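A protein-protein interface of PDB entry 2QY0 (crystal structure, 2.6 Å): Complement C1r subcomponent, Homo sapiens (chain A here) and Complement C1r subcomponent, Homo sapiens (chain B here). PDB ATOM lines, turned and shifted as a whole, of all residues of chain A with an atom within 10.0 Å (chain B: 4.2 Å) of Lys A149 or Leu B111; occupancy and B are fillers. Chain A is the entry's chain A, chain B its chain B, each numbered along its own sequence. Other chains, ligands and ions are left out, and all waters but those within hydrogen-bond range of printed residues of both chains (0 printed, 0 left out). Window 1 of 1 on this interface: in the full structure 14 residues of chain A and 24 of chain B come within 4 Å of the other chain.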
ATOM      1  N   HIS A 103      -6.461  17.813 -34.672  1.00  0.00           N
ATOM      2  CA  HIS A 103      -7.279  18.959 -34.332  1.00  0.00           C
ATOM      3  C   HIS A 103      -6.895  19.470 -32.953  1.00  0.00           C
ATOM      4  O   HIS A 103      -7.442  19.011 -31.935  1.00  0.00           O
ATOM      5  CB  HIS A 103      -8.776  18.570 -34.366  1.00  0.00           C
ATOM      6  CG  HIS A 103      -9.256  18.146 -35.736  1.00  0.00           C
ATOM      7  ND1 HIS A 103     -10.112  17.072 -35.914  1.00  0.00           N
ATOM      8  CD2 HIS A 103      -8.946  18.589 -36.966  1.00  0.00           C
ATOM      9  CE1 HIS A 103     -10.328  16.923 -37.223  1.00  0.00           C
ATOM     10  NE2 HIS A 103      -9.631  17.837 -37.878  1.00  0.00           N
ATOM     11  N   GLU A 104      -5.983  20.424 -32.923  1.00  0.00           N
ATOM     12  CA  GLU A 104      -5.569  21.066 -31.675  1.00  0.00           C
ATOM     13  C   GLU A 104      -6.550  22.210 -31.377  1.00  0.00           C
ATOM     14  O   GLU A 104      -7.226  22.701 -32.283  1.00  0.00           O
ATOM     15  CB  GLU A 104      -4.160  21.649 -31.892  1.00  0.00           C
ATOM     16  CG  GLU A 104      -3.101  20.604 -32.157  1.00  0.00           C
ATOM     17  CD  GLU A 104      -2.122  20.449 -30.996  1.00  0.00           C
ATOM     18  OE1 GLU A 104      -0.897  20.599 -31.261  1.00  0.00           O
ATOM     19  OE2 GLU A 104      -2.576  20.227 -29.842  1.00  0.00           O
ATOM     20  N   PRO A 105      -6.684  22.603 -30.091  1.00  0.00           N
ATOM     21  CA  PRO A 105      -6.076  22.080 -28.848  1.00  0.00           C
ATOM     22  C   PRO A 105      -6.873  20.919 -28.256  1.00  0.00           C
ATOM     23  O   PRO A 105      -6.601  20.472 -27.138  1.00  0.00           O
ATOM     24  CB  PRO A 105      -6.139  23.285 -27.915  1.00  0.00           C
ATOM     25  CG  PRO A 105      -7.399  23.952 -28.292  1.00  0.00           C
ATOM     26  CD  PRO A 105      -7.595  23.711 -29.793  1.00  0.00           C
ATOM     27  N   TYR A 106      -7.845  20.407 -28.994  1.00  0.00           N
ATOM     28  CA  TYR A 106      -8.771  19.429 -28.463  1.00  0.00           C
ATOM     29  C   TYR A 106      -8.157  18.016 -28.505  1.00  0.00           C
ATOM     30  O   TYR A 106      -8.492  17.158 -27.680  1.00  0.00           O
ATOM     31  CB  TYR A 106     -10.079  19.456 -29.258  1.00  0.00           C
ATOM     32  CG  TYR A 106     -10.612  20.833 -29.552  1.00  0.00           C
ATOM     33  CD1 TYR A 106     -10.817  21.259 -30.864  1.00  0.00           C
ATOM     34  CD2 TYR A 106     -10.836  21.745 -28.510  1.00  0.00           C
ATOM     35  CE1 TYR A 106     -11.281  22.538 -31.130  1.00  0.00           C
ATOM     36  CE2 TYR A 106     -11.302  23.034 -28.771  1.00  0.00           C
ATOM     37  CZ  TYR A 106     -11.525  23.415 -30.083  1.00  0.00           C
ATOM     38  OH  TYR A 106     -11.994  24.705 -30.310  1.00  0.00           O
ATOM     39  N   TYR A 107      -7.299  17.822 -29.473  1.00  0.00           N
ATOM     40  CA  TYR A 107      -6.571  16.553 -29.650  1.00  0.00           C
ATOM     41  C   TYR A 107      -5.090  16.860 -29.771  1.00  0.00           C
ATOM     42  O   TYR A 107      -4.723  17.968 -30.157  1.00  0.00           O
ATOM     43  CB  TYR A 107      -7.024  15.811 -30.914  1.00  0.00           C
ATOM     44  CG  TYR A 107      -8.442  15.338 -30.849  1.00  0.00           C
ATOM     45  CD1 TYR A 107      -9.490  16.195 -31.222  1.00  0.00           C
ATOM     46  CD2 TYR A 107      -8.757  14.074 -30.398  1.00  0.00           C
ATOM     47  CE1 TYR A 107     -10.831  15.752 -31.131  1.00  0.00           C
ATOM     48  CE2 TYR A 107     -10.075  13.620 -30.314  1.00  0.00           C
ATOM     49  CZ  TYR A 107     -11.099  14.478 -30.701  1.00  0.00           C
ATOM     50  OH  TYR A 107     -12.407  14.086 -30.612  1.00  0.00           O
ATOM     51  N   LYS A 108      -4.255  15.899 -29.420  1.00  0.00           N
ATOM     52  CA  LYS A 108      -2.794  15.995 -29.489  1.00  0.00           C
ATOM     53  C   LYS A 108      -2.239  14.728 -30.038  1.00  0.00           C
ATOM     54  O   LYS A 108      -2.658  13.655 -29.600  1.00  0.00           O
ATOM     55  CB  LYS A 108      -2.192  16.237 -28.115  1.00  0.00           C
ATOM     56  CG  LYS A 108      -0.668  16.336 -28.109  1.00  0.00           C
ATOM     57  CD  LYS A 108      -0.137  16.697 -26.756  1.00  0.00           C
ATOM     58  CE  LYS A 108       1.340  17.043 -26.747  1.00  0.00           C
ATOM     59  NZ  LYS A 108       1.684  17.739 -25.487  1.00  0.00           N
ATOM     60  N   LEU A 144      -5.113  11.907 -29.668  1.00  0.00           N
ATOM     61  CA  LEU A 144      -5.635  11.548 -28.361  1.00  0.00           C
ATOM     62  C   LEU A 144      -6.248  12.763 -27.697  1.00  0.00           C
ATOM     63  O   LEU A 144      -5.714  13.857 -27.808  1.00  0.00           O
ATOM     64  CB  LEU A 144      -4.544  10.973 -27.455  1.00  0.00           C
ATOM     65  CG  LEU A 144      -3.830   9.701 -27.969  1.00  0.00           C
ATOM     66  CD1 LEU A 144      -2.756   9.272 -26.999  1.00  0.00           C
ATOM     67  CD2 LEU A 144      -4.834   8.589 -28.254  1.00  0.00           C
ATOM     68  N   PRO A 145      -7.379  12.558 -27.029  1.00  0.00           N
ATOM     69  CA  PRO A 145      -8.007  13.568 -26.246  1.00  0.00           C
ATOM     70  C   PRO A 145      -7.087  14.289 -25.272  1.00  0.00           C
ATOM     71  O   PRO A 145      -6.371  13.630 -24.488  1.00  0.00           O
ATOM     72  CB  PRO A 145      -9.035  12.774 -25.427  1.00  0.00           C
ATOM     73  CG  PRO A 145      -9.347  11.611 -26.268  1.00  0.00           C
ATOM     74  CD  PRO A 145      -8.129  11.295 -27.013  1.00  0.00           C
ATOM     75  N   VAL A 146      -7.104  15.618 -25.286  1.00  0.00           N
ATOM     76  CA  VAL A 146      -6.376  16.465 -24.330  1.00  0.00           C
ATOM     77  C   VAL A 146      -7.328  16.799 -23.195  1.00  0.00           C
ATOM     78  O   VAL A 146      -8.484  17.177 -23.419  1.00  0.00           O
ATOM     79  CB  VAL A 146      -5.956  17.804 -25.001  1.00  0.00           C
ATOM     80  CG1 VAL A 146      -5.486  18.795 -23.953  1.00  0.00           C
ATOM     81  CG2 VAL A 146      -4.878  17.558 -26.034  1.00  0.00           C
ATOM     82  N   CYS A 147      -6.861  16.708 -21.968  1.00  0.00           N
ATOM     83  CA  CYS A 147      -7.697  16.941 -20.824  1.00  0.00           C
ATOM     84  C   CYS A 147      -7.377  18.255 -20.101  1.00  0.00           C
ATOM     85  O   CYS A 147      -6.232  18.695 -20.089  1.00  0.00           O
ATOM     86  CB  CYS A 147      -7.629  15.752 -19.838  1.00  0.00           C
ATOM     87  SG  CYS A 147      -6.112  15.600 -18.832  1.00  0.00           S
ATOM     88  N   GLY A 148      -8.400  18.838 -19.476  1.00  0.00           N
ATOM     89  CA  GLY A 148      -8.190  19.976 -18.606  1.00  0.00           C
ATOM     90  C   GLY A 148      -7.752  21.280 -19.242  1.00  0.00           C
ATOM     91  O   GLY A 148      -7.243  22.130 -18.532  1.00  0.00           O
ATOM     92  N   LYS A 149      -7.930  21.453 -20.543  1.00  0.00           N
ATOM     93  CA  LYS A 149      -7.558  22.735 -21.185  1.00  0.00           C
ATOM     94  C   LYS A 149      -8.764  23.373 -21.869  1.00  0.00           C
ATOM     95  O   LYS A 149      -8.880  23.374 -23.085  1.00  0.00           O
ATOM     96  CB  LYS A 149      -6.432  22.556 -22.169  1.00  0.00           C
ATOM     97  CG  LYS A 149      -5.097  22.372 -21.495  1.00  0.00           C
ATOM     98  CD  LYS A 149      -3.916  22.460 -22.460  1.00  0.00           C
ATOM     99  CE  LYS A 149      -2.576  22.520 -21.688  1.00  0.00           C
ATOM    100  NZ  LYS A 149      -2.643  23.389 -20.459  1.00  0.00           N
ATOM    101  N   PRO A 150      -9.669  23.950 -21.052  1.00  0.00           N
ATOM    102  CA  PRO A 150     -10.837  24.575 -21.666  1.00  0.00           C
ATOM    103  C   PRO A 150     -10.422  25.759 -22.481  1.00  0.00           C
ATOM    104  O   PRO A 150      -9.409  26.374 -22.191  1.00  0.00           O
ATOM    105  CB  PRO A 150     -11.713  24.975 -20.466  1.00  0.00           C
ATOM    106  CG  PRO A 150     -10.904  24.678 -19.240  1.00  0.00           C
ATOM    107  CD  PRO A 150      -9.679  23.992 -19.589  1.00  0.00           C
ATOM    108  N   VAL A 151     -11.184  26.075 -23.538  1.00  0.00           N
ATOM    109  CA  VAL A 151     -10.857  27.206 -24.435  1.00  0.00           C
ATOM    110  C   VAL A 151     -11.431  28.484 -23.837  1.00  0.00           C
ATOM    111  O   VAL A 151     -10.861  29.555 -24.039  1.00  0.00           O
ATOM    112  CB  VAL A 151     -11.318  27.031 -25.920  1.00  0.00           C
ATOM    113  CG1 VAL A 151     -10.982  25.644 -26.403  1.00  0.00           C
ATOM    114  CG2 VAL A 151     -12.793  27.315 -26.064  1.00  0.00           C
ATOM    115  N   ASN A 152     -12.564  28.379 -23.113  1.00  0.00           N
ATOM    116  CA  ASN A 152     -13.158  29.526 -22.440  1.00  0.00           C
ATOM    117  C   ASN A 152     -13.245  29.332 -20.919  1.00  0.00           C
ATOM    118  O   ASN A 152     -14.319  29.319 -20.345  1.00  0.00           O
ATOM    119  CB  ASN A 152     -14.531  29.828 -23.056  1.00  0.00           C
ATOM    120  CG  ASN A 152     -15.099  31.162 -22.611  1.00  0.00           C
ATOM    121  OD1 ASN A 152     -14.390  31.996 -22.048  1.00  0.00           O
ATOM    122  ND2 ASN A 152     -16.392  31.396 -22.872  1.00  0.00           N
ATOM    123  N   PRO A 153     -12.100  29.203 -20.272  1.00  0.00           N
ATOM    124  CA  PRO A 153     -12.042  28.873 -18.832  1.00  0.00           C
ATOM    125  C   PRO A 153     -12.438  30.037 -17.939  1.00  0.00           C
ATOM    126  O   PRO A 153     -12.450  31.175 -18.365  1.00  0.00           O
ATOM    127  CB  PRO A 153     -10.574  28.488 -18.624  1.00  0.00           C
ATOM    128  CG  PRO A 153      -9.842  29.281 -19.630  1.00  0.00           C
ATOM    129  CD  PRO A 153     -10.748  29.413 -20.821  1.00  0.00           C
ATOM    130  N   VAL A 154     -12.793  29.767 -16.688  1.00  0.00           N
ATOM    131  CA  VAL A 154     -13.343  30.769 -15.781  1.00  0.00           C
ATOM    132  C   VAL A 154     -12.240  31.662 -15.218  1.00  0.00           C
ATOM    133  O   VAL A 154     -12.429  32.847 -15.035  1.00  0.00           O
ATOM    134  CB  VAL A 154     -14.132  30.140 -14.640  1.00  0.00           C
ATOM    135  CG1 VAL A 154     -14.426  31.132 -13.572  1.00  0.00           C
ATOM    136  CG2 VAL A 154     -15.412  29.528 -15.179  1.00  0.00           C
ATOM    137  N   GLU A 155     -11.108  31.033 -14.922  1.00  0.00           N
ATOM    138  CA  GLU A 155      -9.881  31.724 -14.659  1.00  0.00           C
ATOM    139  C   GLU A 155      -8.792  31.094 -15.539  1.00  0.00           C
ATOM    140  O   GLU A 155      -8.925  29.952 -15.955  1.00  0.00           O
ATOM    141  CB  GLU A 155      -9.516  31.700 -13.148  1.00  0.00           C
ATOM    142  CG  GLU A 155      -9.434  30.290 -12.508  1.00  0.00           C
ATOM    143  CD  GLU A 155      -9.413  30.337 -10.945  1.00  0.00           C
ATOM    144  OE1 GLU A 155      -8.786  29.457 -10.320  1.00  0.00           O
ATOM    145  OE2 GLU A 155     -10.020  31.236 -10.366  1.00  0.00           O
ATOM    146  N   GLN A 156      -7.785  31.856 -15.902  1.00  0.00           N
ATOM    147  CA  GLN A 156      -6.609  31.302 -16.561  1.00  0.00           C
ATOM    148  C   GLN A 156      -5.402  32.202 -16.374  1.00  0.00           C
ATOM    149  O   GLN A 156      -5.560  33.402 -16.069  1.00  0.00           O
ATOM    150  CB  GLN A 156      -6.827  31.036 -18.052  1.00  0.00           C
ATOM    151  CG  GLN A 156      -7.121  32.269 -18.888  1.00  0.00           C
ATOM    152  CD  GLN A 156      -6.814  32.054 -20.372  1.00  0.00           C
ATOM    153  OE1 GLN A 156      -7.358  32.752 -21.232  1.00  0.00           O
ATOM    154  NE2 GLN A 156      -5.930  31.105 -20.694  1.00  0.00           N
ATOM    155  N   ARG A 157      -4.219  31.655 -16.567  1.00  0.00           N
ATOM    156  CA  ARG A 157      -3.065  32.505 -16.421  1.00  0.00           C
ATOM    157  C   ARG A 157      -2.748  33.278 -17.685  1.00  0.00           C
ATOM    158  O   ARG A 157      -3.015  32.826 -18.796  1.00  0.00           O
ATOM    159  CB  ARG A 157      -1.855  31.699 -15.940  1.00  0.00           C
ATOM    160  CG  ARG A 157      -1.450  30.549 -16.775  1.00  0.00           C
ATOM    161  CD  ARG A 157      -0.424  29.749 -16.065  1.00  0.00           C
ATOM    162  NE  ARG A 157       0.204  28.810 -16.983  1.00  0.00           N
ATOM    163  CZ  ARG A 157       1.088  27.879 -16.651  1.00  0.00           C
ATOM    164  NH1 ARG A 157       1.450  27.705 -15.394  1.00  0.00           N
ATOM    165  NH2 ARG A 157       1.584  27.094 -17.580  1.00  0.00           N
ATOM    166  N   PRO B  13     -16.416  22.511 -20.096  1.00  0.00           N
ATOM    167  CA  PRO B  13     -16.660  21.636 -21.249  1.00  0.00           C
ATOM    168  C   PRO B  13     -16.775  20.116 -20.953  1.00  0.00           C
ATOM    169  O   PRO B  13     -17.301  19.367 -21.802  1.00  0.00           O
ATOM    170  CB  PRO B  13     -15.440  21.879 -22.153  1.00  0.00           C
ATOM    171  CG  PRO B  13     -14.390  22.303 -21.202  1.00  0.00           C
ATOM    172  CD  PRO B  13     -15.102  23.163 -20.194  1.00  0.00           C
ATOM    173  N   TRP B  14     -16.320  19.685 -19.794  1.00  0.00           N
ATOM    174  CA  TRP B  14     -16.491  18.277 -19.368  1.00  0.00           C
ATOM    175  C   TRP B  14     -17.843  18.010 -18.728  1.00  0.00           C
ATOM    176  O   TRP B  14     -18.122  16.849 -18.358  1.00  0.00           O
ATOM    177  CB  TRP B  14     -15.438  17.927 -18.348  1.00  0.00           C
ATOM    178  CG  TRP B  14     -15.358  18.923 -17.246  1.00  0.00           C
ATOM    179  CD1 TRP B  14     -16.145  18.987 -16.177  1.00  0.00           C
ATOM    180  CD2 TRP B  14     -14.421  20.017 -17.148  1.00  0.00           C
ATOM    181  NE1 TRP B  14     -15.777  20.062 -15.370  1.00  0.00           N
ATOM    182  CE2 TRP B  14     -14.730  20.709 -15.976  1.00  0.00           C
ATOM    183  CE3 TRP B  14     -13.387  20.479 -17.959  1.00  0.00           C
ATOM    184  CZ2 TRP B  14     -14.014  21.862 -15.569  1.00  0.00           C
ATOM    185  CZ3 TRP B  14     -12.671  21.615 -17.571  1.00  0.00           C
ATOM    186  CH2 TRP B  14     -12.990  22.283 -16.402  1.00  0.00           C
ATOM    187  N   LEU B  28     -16.876  14.396 -18.215  1.00  0.00           N
ATOM    188  CA  LEU B  28     -16.285  13.564 -19.269  1.00  0.00           C
ATOM    189  C   LEU B  28     -14.832  13.240 -18.935  1.00  0.00           C
ATOM    190  O   LEU B  28     -14.115  14.121 -18.516  1.00  0.00           O
ATOM    191  CB  LEU B  28     -16.336  14.334 -20.607  1.00  0.00           C
ATOM    192  CG  LEU B  28     -15.756  13.674 -21.876  1.00  0.00           C
ATOM    193  CD1 LEU B  28     -16.632  12.489 -22.326  1.00  0.00           C
ATOM    194  CD2 LEU B  28     -15.696  14.707 -22.978  1.00  0.00           C
ATOM    195  N   LEU B 106     -14.513  15.800 -29.777  1.00  0.00           N
ATOM    196  CA  LEU B 106     -14.211  16.932 -28.884  1.00  0.00           C
ATOM    197  C   LEU B 106     -14.240  18.256 -29.652  1.00  0.00           C
ATOM    198  O   LEU B 106     -13.996  18.277 -30.847  1.00  0.00           O
ATOM    199  CB  LEU B 106     -12.853  16.742 -28.167  1.00  0.00           C
ATOM    200  CG  LEU B 106     -12.782  15.409 -27.418  1.00  0.00           C
ATOM    201  CD1 LEU B 106     -11.526  15.262 -26.605  1.00  0.00           C
ATOM    202  CD2 LEU B 106     -14.010  15.236 -26.509  1.00  0.00           C
ATOM    203  N   GLY B 107     -14.574  19.296 -28.929  1.00  0.00           N
ATOM    204  CA  GLY B 107     -14.679  20.657 -29.448  1.00  0.00           C
ATOM    205  C   GLY B 107     -14.579  21.686 -28.352  1.00  0.00           C
ATOM    206  O   GLY B 107     -14.371  21.328 -27.160  1.00  0.00           O
ATOM    207  N   LEU B 110     -16.822  20.862 -25.507  1.00  0.00           N
ATOM    208  CA  LEU B 110     -16.827  19.481 -25.058  1.00  0.00           C
ATOM    209  C   LEU B 110     -15.381  18.919 -25.015  1.00  0.00           C
ATOM    210  O   LEU B 110     -14.813  18.587 -26.050  1.00  0.00           O
ATOM    211  CB  LEU B 110     -17.716  18.628 -25.971  1.00  0.00           C
ATOM    212  CG  LEU B 110     -17.925  17.164 -25.558  1.00  0.00           C
ATOM    213  CD1 LEU B 110     -18.607  17.063 -24.188  1.00  0.00           C
ATOM    214  CD2 LEU B 110     -18.753  16.402 -26.654  1.00  0.00           C
ATOM    215  N   LEU B 111     -14.837  18.881 -23.808  1.00  0.00           N
ATOM    216  CA  LEU B 111     -13.460  18.426 -23.507  1.00  0.00           C
ATOM    217  C   LEU B 111     -13.460  17.750 -22.143  1.00  0.00           C
ATOM    218  O   LEU B 111     -14.196  18.181 -21.275  1.00  0.00           O
ATOM    219  CB  LEU B 111     -12.532  19.597 -23.442  1.00  0.00           C
ATOM    220  CG  LEU B 111     -12.477  20.566 -24.643  1.00  0.00           C
ATOM    221  CD1 LEU B 111     -11.814  21.892 -24.236  1.00  0.00           C
ATOM    222  CD2 LEU B 111     -11.741  19.883 -25.794  1.00  0.00           C
ATOM    223  N   PRO B 112     -12.585  16.752 -21.975  1.00  0.00           N
ATOM    224  CA  PRO B 112     -12.547  16.051 -20.668  1.00  0.00           C
ATOM    225  C   PRO B 112     -11.711  16.780 -19.631  1.00  0.00           C
ATOM    226  O   PRO B 112     -10.921  17.707 -19.953  1.00  0.00           O
ATOM    227  CB  PRO B 112     -11.900  14.710 -20.999  1.00  0.00           C
ATOM    228  CG  PRO B 112     -11.002  15.032 -22.135  1.00  0.00           C
ATOM    229  CD  PRO B 112     -11.608  16.174 -22.918  1.00  0.00           C
ATOM    230  N   ILE B 113     -11.884  16.381 -18.400  1.00  0.00           N
ATOM    231  CA  ILE B 113     -11.168  16.943 -17.280  1.00  0.00           C
ATOM    232  C   ILE B 113     -10.095  15.919 -16.911  1.00  0.00           C
ATOM    233  O   ILE B 113     -10.267  14.731 -17.176  1.00  0.00           O
ATOM    234  CB  ILE B 113     -12.110  17.207 -16.070  1.00  0.00           C
ATOM    235  CG1 ILE B 113     -11.428  18.073 -15.000  1.00  0.00           C
ATOM    236  CG2 ILE B 113     -12.617  15.866 -15.486  1.00  0.00           C
ATOM    237  CD1 ILE B 113     -12.406  18.694 -14.010  1.00  0.00           C
ATOM    238  N   ARG B 204      -4.038  23.492 -15.776  1.00  0.00           N
ATOM    239  CA  ARG B 204      -4.869  22.377 -16.177  1.00  0.00           C
ATOM    240  C   ARG B 204      -5.943  22.148 -15.105  1.00  0.00           C
ATOM    241  O   ARG B 204      -5.739  22.444 -13.938  1.00  0.00           O
ATOM    242  CB  ARG B 204      -4.054  21.070 -16.391  1.00  0.00           C
ATOM    243  CG  ARG B 204      -3.251  21.018 -17.715  1.00  0.00           C
ATOM    244  CD  ARG B 204      -2.284  19.805 -17.854  1.00  0.00           C
ATOM    245  NE  ARG B 204      -2.577  18.714 -16.921  1.00  0.00           N
ATOM    246  CZ  ARG B 204      -1.718  18.141 -16.079  1.00  0.00           C
ATOM    247  NH1 ARG B 204      -0.438  18.545 -16.023  1.00  0.00           N
ATOM    248  NH2 ARG B 204      -2.140  17.158 -15.256  1.00  0.00           N
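Among the printed residues, pairs that only touch across the chains: Tyr A106 with Leu B106 (3.7 Å), Tyr A106 with Gly B107 (3.6 Å), Tyr A106 with Leu B111 (3.4 Å), Pro A145 with Leu B106 (3.7 Å), Val A146 with Pro B112 (3.3 Å), Cys A147 with Pro B112 (3.4 Å), Cys A147 with Ile B113 (3.8 Å), Gly A148 with Arg B204 (3.4 Å), Lys A149 with Leu B111 (3.5 Å), Lys A149 with Arg B204 (3.7 Å), Pro A150 with Pro B13 (3.9 Å), Pro A150 with Trp B14 (3.9 Å) and Pro A150 with Leu B111 (3.8 Å).
Of the 10 printed residues of chain B, 8 touch a printed residue of chain A.
Hydrophobic or aromatic side chains of chain B within 4 Å of the printed part of chain A: Pro B13, Trp B14, Leu B106, Leu B111 and Pro B112.
Hydrophobic or aromatic side chains of chain A that line the printed part of chain B: Tyr A106, Tyr A107, Pro A145 and Pro A150.
Among the printed residues, 15 pairs touch across the chains.
Among the printed residues, no Asp or Glu carboxylate lies within 4 Å of a Lys or Arg side-chain nitrogen of the other chain.
OH of Tyr A107 sits at hydrogen-bond distance from N of Leu B106.
N of Gly A148 lies within hydrogen-bond range of O of Pro B112.
Printed residues of chain B within 4 Å of Lys A149: Leu B111 (3.5 Å) and Arg B204 (3.7 Å).
Of the printed residues of chain A, Leu B111 touches Tyr A106, Lys A149 and Pro A150.
Printed residues of chain A within 4 Å of Pro B13: Pro A150.
Gly B107 touches just one residue of chain A: Tyr A106 (3.6 Å).
No residue of chain A comes within 4 Å of Leu B110.
Of the printed residues of chain A, Trp B14 touches Pro A150.
Of the printed residues of chain B, Gly A148 touches Pro B112 and Arg B204.
Printed residues of chain A within 4 Å of Leu B106: Tyr A106, Tyr A107 and Pro A145.
Printed residues of chain A within 4 Å of Ile B113: Cys A147.
The nearest printed residue of chain B that does not touch Lys A149 is Pro B112 (4.8 Å).
The nearest residue of chain A that does not touch Leu B111 is Val A151 (4.3 Å).
The nearest printed residue of chain B that does not touch Cys A147 is Arg B204 (4.5 Å).
The backbone carbonyl oxygen (O) of Tyr A106 is in hydrogen-bond range of the backbone NH (N) of Val A146 (3.2 Å).
O of Pro B13 sits at hydrogen-bond distance from N of Leu B111.
The backbone carbonyl oxygen (O) of Trp B14 sits at hydrogen-bond distance from the backbone NH (N) of Leu B28 (2.8 Å).
The backbone carbonyl oxygen (O) of Leu B111 sits close to the backbone NH (N) of Trp B14, at 3.0 Å.
The backbone carbonyl oxygen (O) of Leu B28 is in hydrogen-bond range of the backbone NH (N) of Ile B113, 3.2 Å away.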
